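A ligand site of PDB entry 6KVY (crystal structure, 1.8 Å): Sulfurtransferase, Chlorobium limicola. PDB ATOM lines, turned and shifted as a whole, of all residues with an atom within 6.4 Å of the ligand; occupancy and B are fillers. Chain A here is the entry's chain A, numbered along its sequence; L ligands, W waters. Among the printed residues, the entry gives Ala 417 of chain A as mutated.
NE of Arg 420 lies close to O of Ala 377. The side-chain hydroxyl of Ser 260 lies within hydrogen-bond range of the backbone carbonyl oxygen of Tyr 191, 2.7 Å away. The guanidinium group (NH2) of Arg 269 lies close to the backbone carbonyl oxygen (O) of Trp 219, 3.1 Å away. The backbone NH (N) of Gly 418 sits at hydrogen-bond distance from SG of CSS 415. The side-chain carboxylate (OE1) of Glu 214 lies within salt-bridge range of the guanidinium group (NE) of Arg 269 (2.8 Å). The backbone NH (N) of Ala 417 lies close to SD of CSS 415 (3.6 Å). The guanidinium group (NH2) of Arg 420 lies within hydrogen-bond range of the side-chain hydroxyl (OH) of Tyr 356, at 2.8 Å. SD of CSS 415 is in hydrogen-bond range of the side-chain hydroxyl of Tyr 356 (3.3 Å).
CE2 of Tyr 191 touches O2 of the ligand (3.6 Å). Glu 214 touches the ligand. CE3 of Trp 219 touches C1 of the ligand (3.4 Å). Gly 259 touches the ligand (CA to O2, 3.4 Å). Trp 419 touches the ligand. Ten residues have an atom within 4 Å of the ligand: Tyr 191, Glu 214, Trp 219, Gly 259, Tyr 356, Tyr 358, Ala 377, Tyr 378, CSS 415 and Trp 419. The nearest printed residue that does not touch the ligand is Arg 420 (4.1 Å).
Water W1 lies within hydrogen-bond range of a nitrogen (N1) of the ligand (2.6 Å), the side-chain hydroxyl of Tyr 356 (2.8 Å), the side-chain hydroxyl of Tyr 358 (3.1 Å), the backbone NH of Ala 417 (3.3 Å) and SD of CSS 415 (3.6 Å). Water W4 bridges an oxygen (O2) of the ligand (2.6 Å) and the backbone NH of Gly 259 (2.9 Å). Water W3 lies within hydrogen-bond range of N of Trp 419 (2.9 Å), N of Gly 418 (3.2 Å), N1 of the ligand (3.5 Å) and SD of CSS 415 (3.5 Å).
OH of Tyr 358 is in hydrogen-bond range of O1 of the ligand (2.7 Å). OH of Tyr 356 sits close to N1 of the ligand, at 3.5 Å. OH of Tyr 378 is in hydrogen-bond range of O1 of the ligand. N1 of the ligand sits close to SD of CSS 415, at 3.7 Å. O of Ala 377 lies close to N2 of the ligand.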
ATOM      1  N   TYR A 191      -9.533  19.724 -33.336  1.00  0.00           N
ATOM      2  CA  TYR A 191     -10.540  20.447 -34.107  1.00  0.00           C
ATOM      3  C   TYR A 191      -9.881  21.652 -34.778  1.00  0.00           C
ATOM      4  O   TYR A 191      -9.498  22.620 -34.114  1.00  0.00           O
ATOM      5  CB  TYR A 191     -11.687  20.904 -33.193  1.00  0.00           C
ATOM      6  CG  TYR A 191     -12.680  21.821 -33.869  1.00  0.00           C
ATOM      7  CD1 TYR A 191     -13.206  21.520 -35.123  1.00  0.00           C
ATOM      8  CD2 TYR A 191     -13.131  22.965 -33.217  1.00  0.00           C
ATOM      9  CE1 TYR A 191     -14.147  22.362 -35.727  1.00  0.00           C
ATOM     10  CE2 TYR A 191     -14.072  23.803 -33.808  1.00  0.00           C
ATOM     11  CZ  TYR A 191     -14.574  23.504 -35.056  1.00  0.00           C
ATOM     12  OH  TYR A 191     -15.501  24.356 -35.621  1.00  0.00           O
ATOM     13  N   THR A 210     -11.074  16.654 -36.357  1.00  0.00           N
ATOM     14  CA  THR A 210     -12.419  16.109 -36.108  1.00  0.00           C
ATOM     15  C   THR A 210     -13.338  16.353 -37.328  1.00  0.00           C
ATOM     16  O   THR A 210     -14.235  15.590 -37.505  1.00  0.00           O
ATOM     17  CB  THR A 210     -12.981  16.634 -34.784  1.00  0.00           C
ATOM     18  OG1 THR A 210     -12.963  18.052 -34.796  1.00  0.00           O
ATOM     19  CG2 THR A 210     -12.176  16.120 -33.606  1.00  0.00           C
ATOM     20  N   LEU A 211     -13.125  17.431 -38.067  1.00  0.00           N
ATOM     21  CA  LEU A 211     -13.885  17.684 -39.318  1.00  0.00           C
ATOM     22  C   LEU A 211     -13.730  16.513 -40.302  1.00  0.00           C
ATOM     23  O   LEU A 211     -14.502  16.488 -41.222  1.00  0.00           O
ATOM     24  CB  LEU A 211     -13.371  18.980 -39.918  1.00  0.00           C
ATOM     25  CG  LEU A 211     -13.795  20.202 -39.137  1.00  0.00           C
ATOM     26  CD1 LEU A 211     -13.066  21.454 -39.559  1.00  0.00           C
ATOM     27  CD2 LEU A 211     -15.281  20.381 -39.213  1.00  0.00           C
ATOM     28  N   GLU A 214     -16.861  14.370 -38.769  1.00  0.00           N
ATOM     29  CA  GLU A 214     -18.146  14.993 -38.483  1.00  0.00           C
ATOM     30  C   GLU A 214     -18.311  16.236 -39.350  1.00  0.00           C
ATOM     31  O   GLU A 214     -17.334  16.884 -39.745  1.00  0.00           O
ATOM     32  CB  GLU A 214     -18.279  15.345 -36.979  1.00  0.00           C
ATOM     33  CG  GLU A 214     -17.399  16.465 -36.485  1.00  0.00           C
ATOM     34  CD  GLU A 214     -17.499  16.678 -34.984  1.00  0.00           C
ATOM     35  OE1 GLU A 214     -18.330  15.990 -34.339  1.00  0.00           O
ATOM     36  OE2 GLU A 214     -16.756  17.526 -34.458  1.00  0.00           O
ATOM     37  N   TRP A 219     -22.954  19.197 -37.311  1.00  0.00           N
ATOM     38  CA  TRP A 219     -22.120  18.691 -36.213  1.00  0.00           C
ATOM     39  C   TRP A 219     -22.483  17.257 -35.837  1.00  0.00           C
ATOM     40  O   TRP A 219     -22.192  16.797 -34.733  1.00  0.00           O
ATOM     41  CB  TRP A 219     -22.145  19.645 -35.011  1.00  0.00           C
ATOM     42  CG  TRP A 219     -21.555  20.992 -35.368  1.00  0.00           C
ATOM     43  CD1 TRP A 219     -22.169  22.218 -35.299  1.00  0.00           C
ATOM     44  CD2 TRP A 219     -20.238  21.241 -35.900  1.00  0.00           C
ATOM     45  NE1 TRP A 219     -21.308  23.209 -35.718  1.00  0.00           N
ATOM     46  CE2 TRP A 219     -20.124  22.637 -36.108  1.00  0.00           C
ATOM     47  CE3 TRP A 219     -19.154  20.414 -36.226  1.00  0.00           C
ATOM     48  CZ2 TRP A 219     -18.971  23.218 -36.621  1.00  0.00           C
ATOM     49  CZ3 TRP A 219     -18.000  21.005 -36.729  1.00  0.00           C
ATOM     50  CH2 TRP A 219     -17.908  22.392 -36.915  1.00  0.00           C
ATOM     51  N   PHE A 257     -12.810  29.560 -31.481  1.00  0.00           N
ATOM     52  CA  PHE A 257     -12.953  28.093 -31.510  1.00  0.00           C
ATOM     53  C   PHE A 257     -12.312  27.493 -30.263  1.00  0.00           C
ATOM     54  O   PHE A 257     -11.202  26.919 -30.332  1.00  0.00           O
ATOM     55  CB  PHE A 257     -12.335  27.502 -32.782  1.00  0.00           C
ATOM     56  CG  PHE A 257     -12.950  28.001 -34.051  1.00  0.00           C
ATOM     57  CD1 PHE A 257     -14.239  27.634 -34.396  1.00  0.00           C
ATOM     58  CD2 PHE A 257     -12.248  28.838 -34.896  1.00  0.00           C
ATOM     59  CE1 PHE A 257     -14.829  28.094 -35.567  1.00  0.00           C
ATOM     60  CE2 PHE A 257     -12.828  29.309 -36.080  1.00  0.00           C
ATOM     61  CZ  PHE A 257     -14.114  28.934 -36.397  1.00  0.00           C
ATOM     62  N   PRO A 258     -12.976  27.587 -29.120  1.00  0.00           N
ATOM     63  CA  PRO A 258     -12.394  26.993 -27.904  1.00  0.00           C
ATOM     64  C   PRO A 258     -12.198  25.494 -28.038  1.00  0.00           C
ATOM     65  O   PRO A 258     -11.325  24.935 -27.361  1.00  0.00           O
ATOM     66  CB  PRO A 258     -13.420  27.340 -26.808  1.00  0.00           C
ATOM     67  CG  PRO A 258     -14.194  28.498 -27.361  1.00  0.00           C
ATOM     68  CD  PRO A 258     -14.261  28.251 -28.846  1.00  0.00           C
ATOM     69  N   GLY A 259     -12.986  24.844 -28.890  1.00  0.00           N
ATOM     70  CA  GLY A 259     -12.857  23.407 -29.092  1.00  0.00           C
ATOM     71  C   GLY A 259     -11.509  23.000 -29.639  1.00  0.00           C
ATOM     72  O   GLY A 259     -11.086  21.852 -29.462  1.00  0.00           O
ATOM     73  N   SER A 260     -10.810  23.938 -30.296  1.00  0.00           N
ATOM     74  CA  SER A 260      -9.471  23.652 -30.804  1.00  0.00           C
ATOM     75  C   SER A 260      -8.495  23.366 -29.687  1.00  0.00           C
ATOM     76  O   SER A 260      -7.428  22.807 -29.940  1.00  0.00           O
ATOM     77  CB  SER A 260      -8.963  24.830 -31.648  1.00  0.00           C
ATOM     78  OG  SER A 260      -9.725  24.951 -32.846  1.00  0.00           O
ATOM     79  N   ALA A 262      -9.616  21.700 -26.789  1.00  0.00           N
ATOM     80  CA  ALA A 262     -10.193  20.587 -26.026  1.00  0.00           C
ATOM     81  C   ALA A 262      -9.922  19.265 -26.756  1.00  0.00           C
ATOM     82  O   ALA A 262     -10.833  18.478 -27.049  1.00  0.00           O
ATOM     83  CB  ALA A 262     -11.675  20.814 -25.810  1.00  0.00           C
ATOM     84  N   ILE A 265     -11.261  15.696 -25.392  1.00  0.00           N
ATOM     85  CA  ILE A 265     -12.677  15.456 -25.665  1.00  0.00           C
ATOM     86  C   ILE A 265     -12.836  15.061 -27.123  1.00  0.00           C
ATOM     87  O   ILE A 265     -13.559  14.117 -27.464  1.00  0.00           O
ATOM     88  CB  ILE A 265     -13.557  16.684 -25.356  1.00  0.00           C
ATOM     89  CG1 ILE A 265     -13.326  17.235 -23.949  1.00  0.00           C
ATOM     90  CG2 ILE A 265     -15.051  16.310 -25.498  1.00  0.00           C
ATOM     91  CD1 ILE A 265     -14.172  18.477 -23.647  1.00  0.00           C
ATOM     92  N   ARG A 269     -14.565  11.801 -28.803  1.00  0.00           N
ATOM     93  CA  ARG A 269     -15.576  11.951 -29.851  1.00  0.00           C
ATOM     94  C   ARG A 269     -15.223  11.111 -31.083  1.00  0.00           C
ATOM     95  O   ARG A 269     -16.081  10.399 -31.616  1.00  0.00           O
ATOM     96  CB  ARG A 269     -15.705  13.430 -30.225  1.00  0.00           C
ATOM     97  CG  ARG A 269     -16.508  13.678 -31.518  1.00  0.00           C
ATOM     98  CD  ARG A 269     -17.980  13.350 -31.356  1.00  0.00           C
ATOM     99  NE  ARG A 269     -18.746  13.923 -32.477  1.00  0.00           N
ATOM    100  CZ  ARG A 269     -20.038  13.695 -32.711  1.00  0.00           C
ATOM    101  NH1 ARG A 269     -20.727  12.887 -31.925  1.00  0.00           N
ATOM    102  NH2 ARG A 269     -20.630  14.277 -33.754  1.00  0.00           N
ATOM    103  N   TYR A 356     -22.180  28.346 -26.424  1.00  0.00           N
ATOM    104  CA  TYR A 356     -21.466  28.351 -27.690  1.00  0.00           C
ATOM    105  C   TYR A 356     -21.636  29.690 -28.392  1.00  0.00           C
ATOM    106  O   TYR A 356     -22.679  30.326 -28.289  1.00  0.00           O
ATOM    107  CB  TYR A 356     -21.989  27.280 -28.622  1.00  0.00           C
ATOM    108  CG  TYR A 356     -21.842  25.888 -28.086  1.00  0.00           C
ATOM    109  CD1 TYR A 356     -20.682  25.161 -28.317  1.00  0.00           C
ATOM    110  CD2 TYR A 356     -22.870  25.302 -27.356  1.00  0.00           C
ATOM    111  CE1 TYR A 356     -20.550  23.878 -27.840  1.00  0.00           C
ATOM    112  CE2 TYR A 356     -22.738  24.005 -26.875  1.00  0.00           C
ATOM    113  CZ  TYR A 356     -21.580  23.299 -27.137  1.00  0.00           C
ATOM    114  OH  TYR A 356     -21.456  22.007 -26.691  1.00  0.00           O
ATOM    115  N   TYR A 358     -21.930  29.797 -31.541  1.00  0.00           N
ATOM    116  CA  TYR A 358     -22.661  29.452 -32.756  1.00  0.00           C
ATOM    117  C   TYR A 358     -24.044  28.894 -32.470  1.00  0.00           C
ATOM    118  O   TYR A 358     -24.697  28.356 -33.375  1.00  0.00           O
ATOM    119  CB  TYR A 358     -21.854  28.462 -33.619  1.00  0.00           C
ATOM    120  CG  TYR A 358     -21.470  27.174 -32.926  1.00  0.00           C
ATOM    121  CD1 TYR A 358     -22.310  26.059 -32.944  1.00  0.00           C
ATOM    122  CD2 TYR A 358     -20.226  27.050 -32.283  1.00  0.00           C
ATOM    123  CE1 TYR A 358     -21.936  24.859 -32.308  1.00  0.00           C
ATOM    124  CE2 TYR A 358     -19.852  25.864 -31.650  1.00  0.00           C
ATOM    125  CZ  TYR A 358     -20.710  24.776 -31.675  1.00  0.00           C
ATOM    126  OH  TYR A 358     -20.325  23.591 -31.064  1.00  0.00           O
ATOM    127  N   ALA A 377     -18.851  24.335 -21.830  1.00  0.00           N
ATOM    128  CA  ALA A 377     -18.933  23.355 -22.907  1.00  0.00           C
ATOM    129  C   ALA A 377     -17.587  22.724 -23.228  1.00  0.00           C
ATOM    130  O   ALA A 377     -17.562  21.714 -23.932  1.00  0.00           O
ATOM    131  CB  ALA A 377     -19.523  24.006 -24.159  1.00  0.00           C
ATOM    132  N   TYR A 378     -16.483  23.278 -22.725  1.00  0.00           N
ATOM    133  CA  TYR A 378     -15.161  22.838 -23.148  1.00  0.00           C
ATOM    134  C   TYR A 378     -14.348  22.218 -22.013  1.00  0.00           C
ATOM    135  O   TYR A 378     -13.134  22.000 -22.178  1.00  0.00           O
ATOM    136  CB  TYR A 378     -14.437  24.044 -23.794  1.00  0.00           C
ATOM    137  CG  TYR A 378     -15.182  24.524 -25.015  1.00  0.00           C
ATOM    138  CD1 TYR A 378     -15.109  23.830 -26.210  1.00  0.00           C
ATOM    139  CD2 TYR A 378     -16.005  25.657 -24.956  1.00  0.00           C
ATOM    140  CE1 TYR A 378     -15.812  24.234 -27.336  1.00  0.00           C
ATOM    141  CE2 TYR A 378     -16.715  26.083 -26.083  1.00  0.00           C
ATOM    142  CZ  TYR A 378     -16.612  25.368 -27.271  1.00  0.00           C
ATOM    143  OH  TYR A 378     -17.310  25.765 -28.400  1.00  0.00           O
ATOM    144  N   HIS A 379     -14.988  21.881 -20.892  1.00  0.00           N
ATOM    145  CA  HIS A 379     -14.319  21.260 -19.755  1.00  0.00           C
ATOM    146  C   HIS A 379     -15.206  20.159 -19.202  1.00  0.00           C
ATOM    147  O   HIS A 379     -16.439  20.306 -19.135  1.00  0.00           O
ATOM    148  CB  HIS A 379     -14.026  22.289 -18.643  1.00  0.00           C
ATOM    149  CG  HIS A 379     -13.084  23.374 -19.065  1.00  0.00           C
ATOM    150  ND1 HIS A 379     -13.499  24.481 -19.775  1.00  0.00           N
ATOM    151  CD2 HIS A 379     -11.745  23.515 -18.887  1.00  0.00           C
ATOM    152  CE1 HIS A 379     -12.454  25.256 -20.023  1.00  0.00           C
ATOM    153  NE2 HIS A 379     -11.377  24.697 -19.492  1.00  0.00           N
ATOM    154  N   CSS A 415     -25.211  16.411 -25.603  1.00  0.00           N
ATOM    155  CA  CSS A 415     -24.728  17.675 -25.094  1.00  0.00           C
ATOM    156  CB  CSS A 415     -23.221  17.675 -24.818  1.00  0.00           C
ATOM    157  SG  CSS A 415     -22.286  17.113 -26.192  1.00  0.00           S
ATOM    158  SD  CSS A 415     -21.015  18.738 -26.670  1.00  0.00           S
ATOM    159  C   CSS A 415     -25.098  18.715 -26.133  1.00  0.00           C
ATOM    160  O   CSS A 415     -26.187  18.703 -26.720  1.00  0.00           O
ATOM    161  N   GLY A 416     -24.162  19.632 -26.394  1.00  0.00           N
ATOM    162  CA  GLY A 416     -24.398  20.649 -27.419  1.00  0.00           C
ATOM    163  C   GLY A 416     -24.512  20.020 -28.797  1.00  0.00           C
ATOM    164  O   GLY A 416     -25.477  20.255 -29.532  1.00  0.00           O
ATOM    165  N   ALA A 417     -23.506  19.226 -29.160  1.00  0.00           N
ATOM    166  CA  ALA A 417     -23.488  18.624 -30.495  1.00  0.00           C
ATOM    167  C   ALA A 417     -22.775  17.269 -30.532  1.00  0.00           C
ATOM    168  O   ALA A 417     -22.467  16.782 -31.622  1.00  0.00           O
ATOM    169  CB  ALA A 417     -22.827  19.575 -31.513  1.00  0.00           C
ATOM    170  N   GLY A 418     -22.487  16.653 -29.382  1.00  0.00           N
ATOM    171  CA  GLY A 418     -22.052  15.269 -29.348  1.00  0.00           C
ATOM    172  C   GLY A 418     -20.694  15.013 -28.712  1.00  0.00           C
ATOM    173  O   GLY A 418     -20.395  13.853 -28.412  1.00  0.00           O
ATOM    174  N   TRP A 419     -19.848  16.028 -28.523  1.00  0.00           N
ATOM    175  CA  TRP A 419     -18.508  15.766 -27.990  1.00  0.00           C
ATOM    176  C   TRP A 419     -18.545  15.340 -26.524  1.00  0.00           C
ATOM    177  O   TRP A 419     -18.043  14.275 -26.154  1.00  0.00           O
ATOM    178  CB  TRP A 419     -17.614  17.003 -28.119  1.00  0.00           C
ATOM    179  CG  TRP A 419     -16.925  17.194 -29.429  1.00  0.00           C
ATOM    180  CD1 TRP A 419     -17.416  16.930 -30.683  1.00  0.00           C
ATOM    181  CD2 TRP A 419     -15.610  17.721 -29.608  1.00  0.00           C
ATOM    182  NE1 TRP A 419     -16.475  17.273 -31.633  1.00  0.00           N
ATOM    183  CE2 TRP A 419     -15.356  17.746 -30.998  1.00  0.00           C
ATOM    184  CE3 TRP A 419     -14.624  18.186 -28.725  1.00  0.00           C
ATOM    185  CZ2 TRP A 419     -14.147  18.220 -31.529  1.00  0.00           C
ATOM    186  CZ3 TRP A 419     -13.426  18.662 -29.246  1.00  0.00           C
ATOM    187  CH2 TRP A 419     -13.195  18.671 -30.639  1.00  0.00           C
ATOM    188  N   ARG A 420     -19.092  16.196 -25.656  1.00  0.00           N
ATOM    189  CA  ARG A 420     -19.131  15.860 -24.239  1.00  0.00           C
ATOM    190  C   ARG A 420     -19.949  14.607 -24.010  1.00  0.00           C
ATOM    191  O   ARG A 420     -19.581  13.768 -23.174  1.00  0.00           O
ATOM    192  CB  ARG A 420     -19.715  17.023 -23.426  1.00  0.00           C
ATOM    193  CG  ARG A 420     -18.832  18.252 -23.395  1.00  0.00           C
ATOM    194  CD  ARG A 420     -19.552  19.382 -22.698  1.00  0.00           C
ATOM    195  NE  ARG A 420     -20.567  19.981 -23.575  1.00  0.00           N
ATOM    196  CZ  ARG A 420     -21.425  20.919 -23.177  1.00  0.00           C
ATOM    197  NH1 ARG A 420     -21.408  21.340 -21.914  1.00  0.00           N
ATOM    198  NH2 ARG A 420     -22.300  21.435 -24.041  1.00  0.00           N
HETATM  199  C1  LIG L   1     -18.483  20.265 -32.902  1.00  0.00           C
HETATM  200  C2  LIG L   1     -16.135  20.956 -32.985  1.00  0.00           C
HETATM  201  C3  LIG L   1     -17.910  22.657 -33.324  1.00  0.00           C
HETATM  202  O1  LIG L   1     -17.832  23.889 -30.140  1.00  0.00           O
HETATM  203  O2  LIG L   1     -15.808  23.121 -30.758  1.00  0.00           O
HETATM  204  C4  LIG L   1     -16.314  20.766 -27.625  1.00  0.00           C
HETATM  205  C5  LIG L   1     -16.975  20.601 -30.131  1.00  0.00           C
HETATM  206  N1  LIG L   1     -18.451  20.951 -28.130  1.00  0.00           N
HETATM  207  N2  LIG L   1     -17.016  20.945 -26.435  1.00  0.00           N
HETATM  208  C6  LIG L   1     -17.064  23.082 -30.592  1.00  0.00           C
HETATM  209  C7  LIG L   1     -17.229  20.760 -28.684  1.00  0.00           C
HETATM  210  C8  LIG L   1     -18.342  21.081 -26.782  1.00  0.00           C
HETATM  211  C9  LIG L   1     -17.666  21.654 -30.968  1.00  0.00           C
HETATM  212  N3  LIG L   1     -17.549  21.391 -32.550  1.00  0.00           N
HETATM  213  O   HOH W   1     -20.801  21.151 -29.276  1.00  0.00           O
HETATM  214  O   HOH W   2     -19.990  17.665 -32.822  1.00  0.00           O
HETATM  215  O   HOH W   3     -20.008  18.497 -30.061  1.00  0.00           O
HETATM  216  O   HOH W   4     -14.864  25.580 -30.924  1.00  0.00           O
HETATM  217  O   HOH W   5     -17.119  25.770 -33.906  1.00  0.00           O
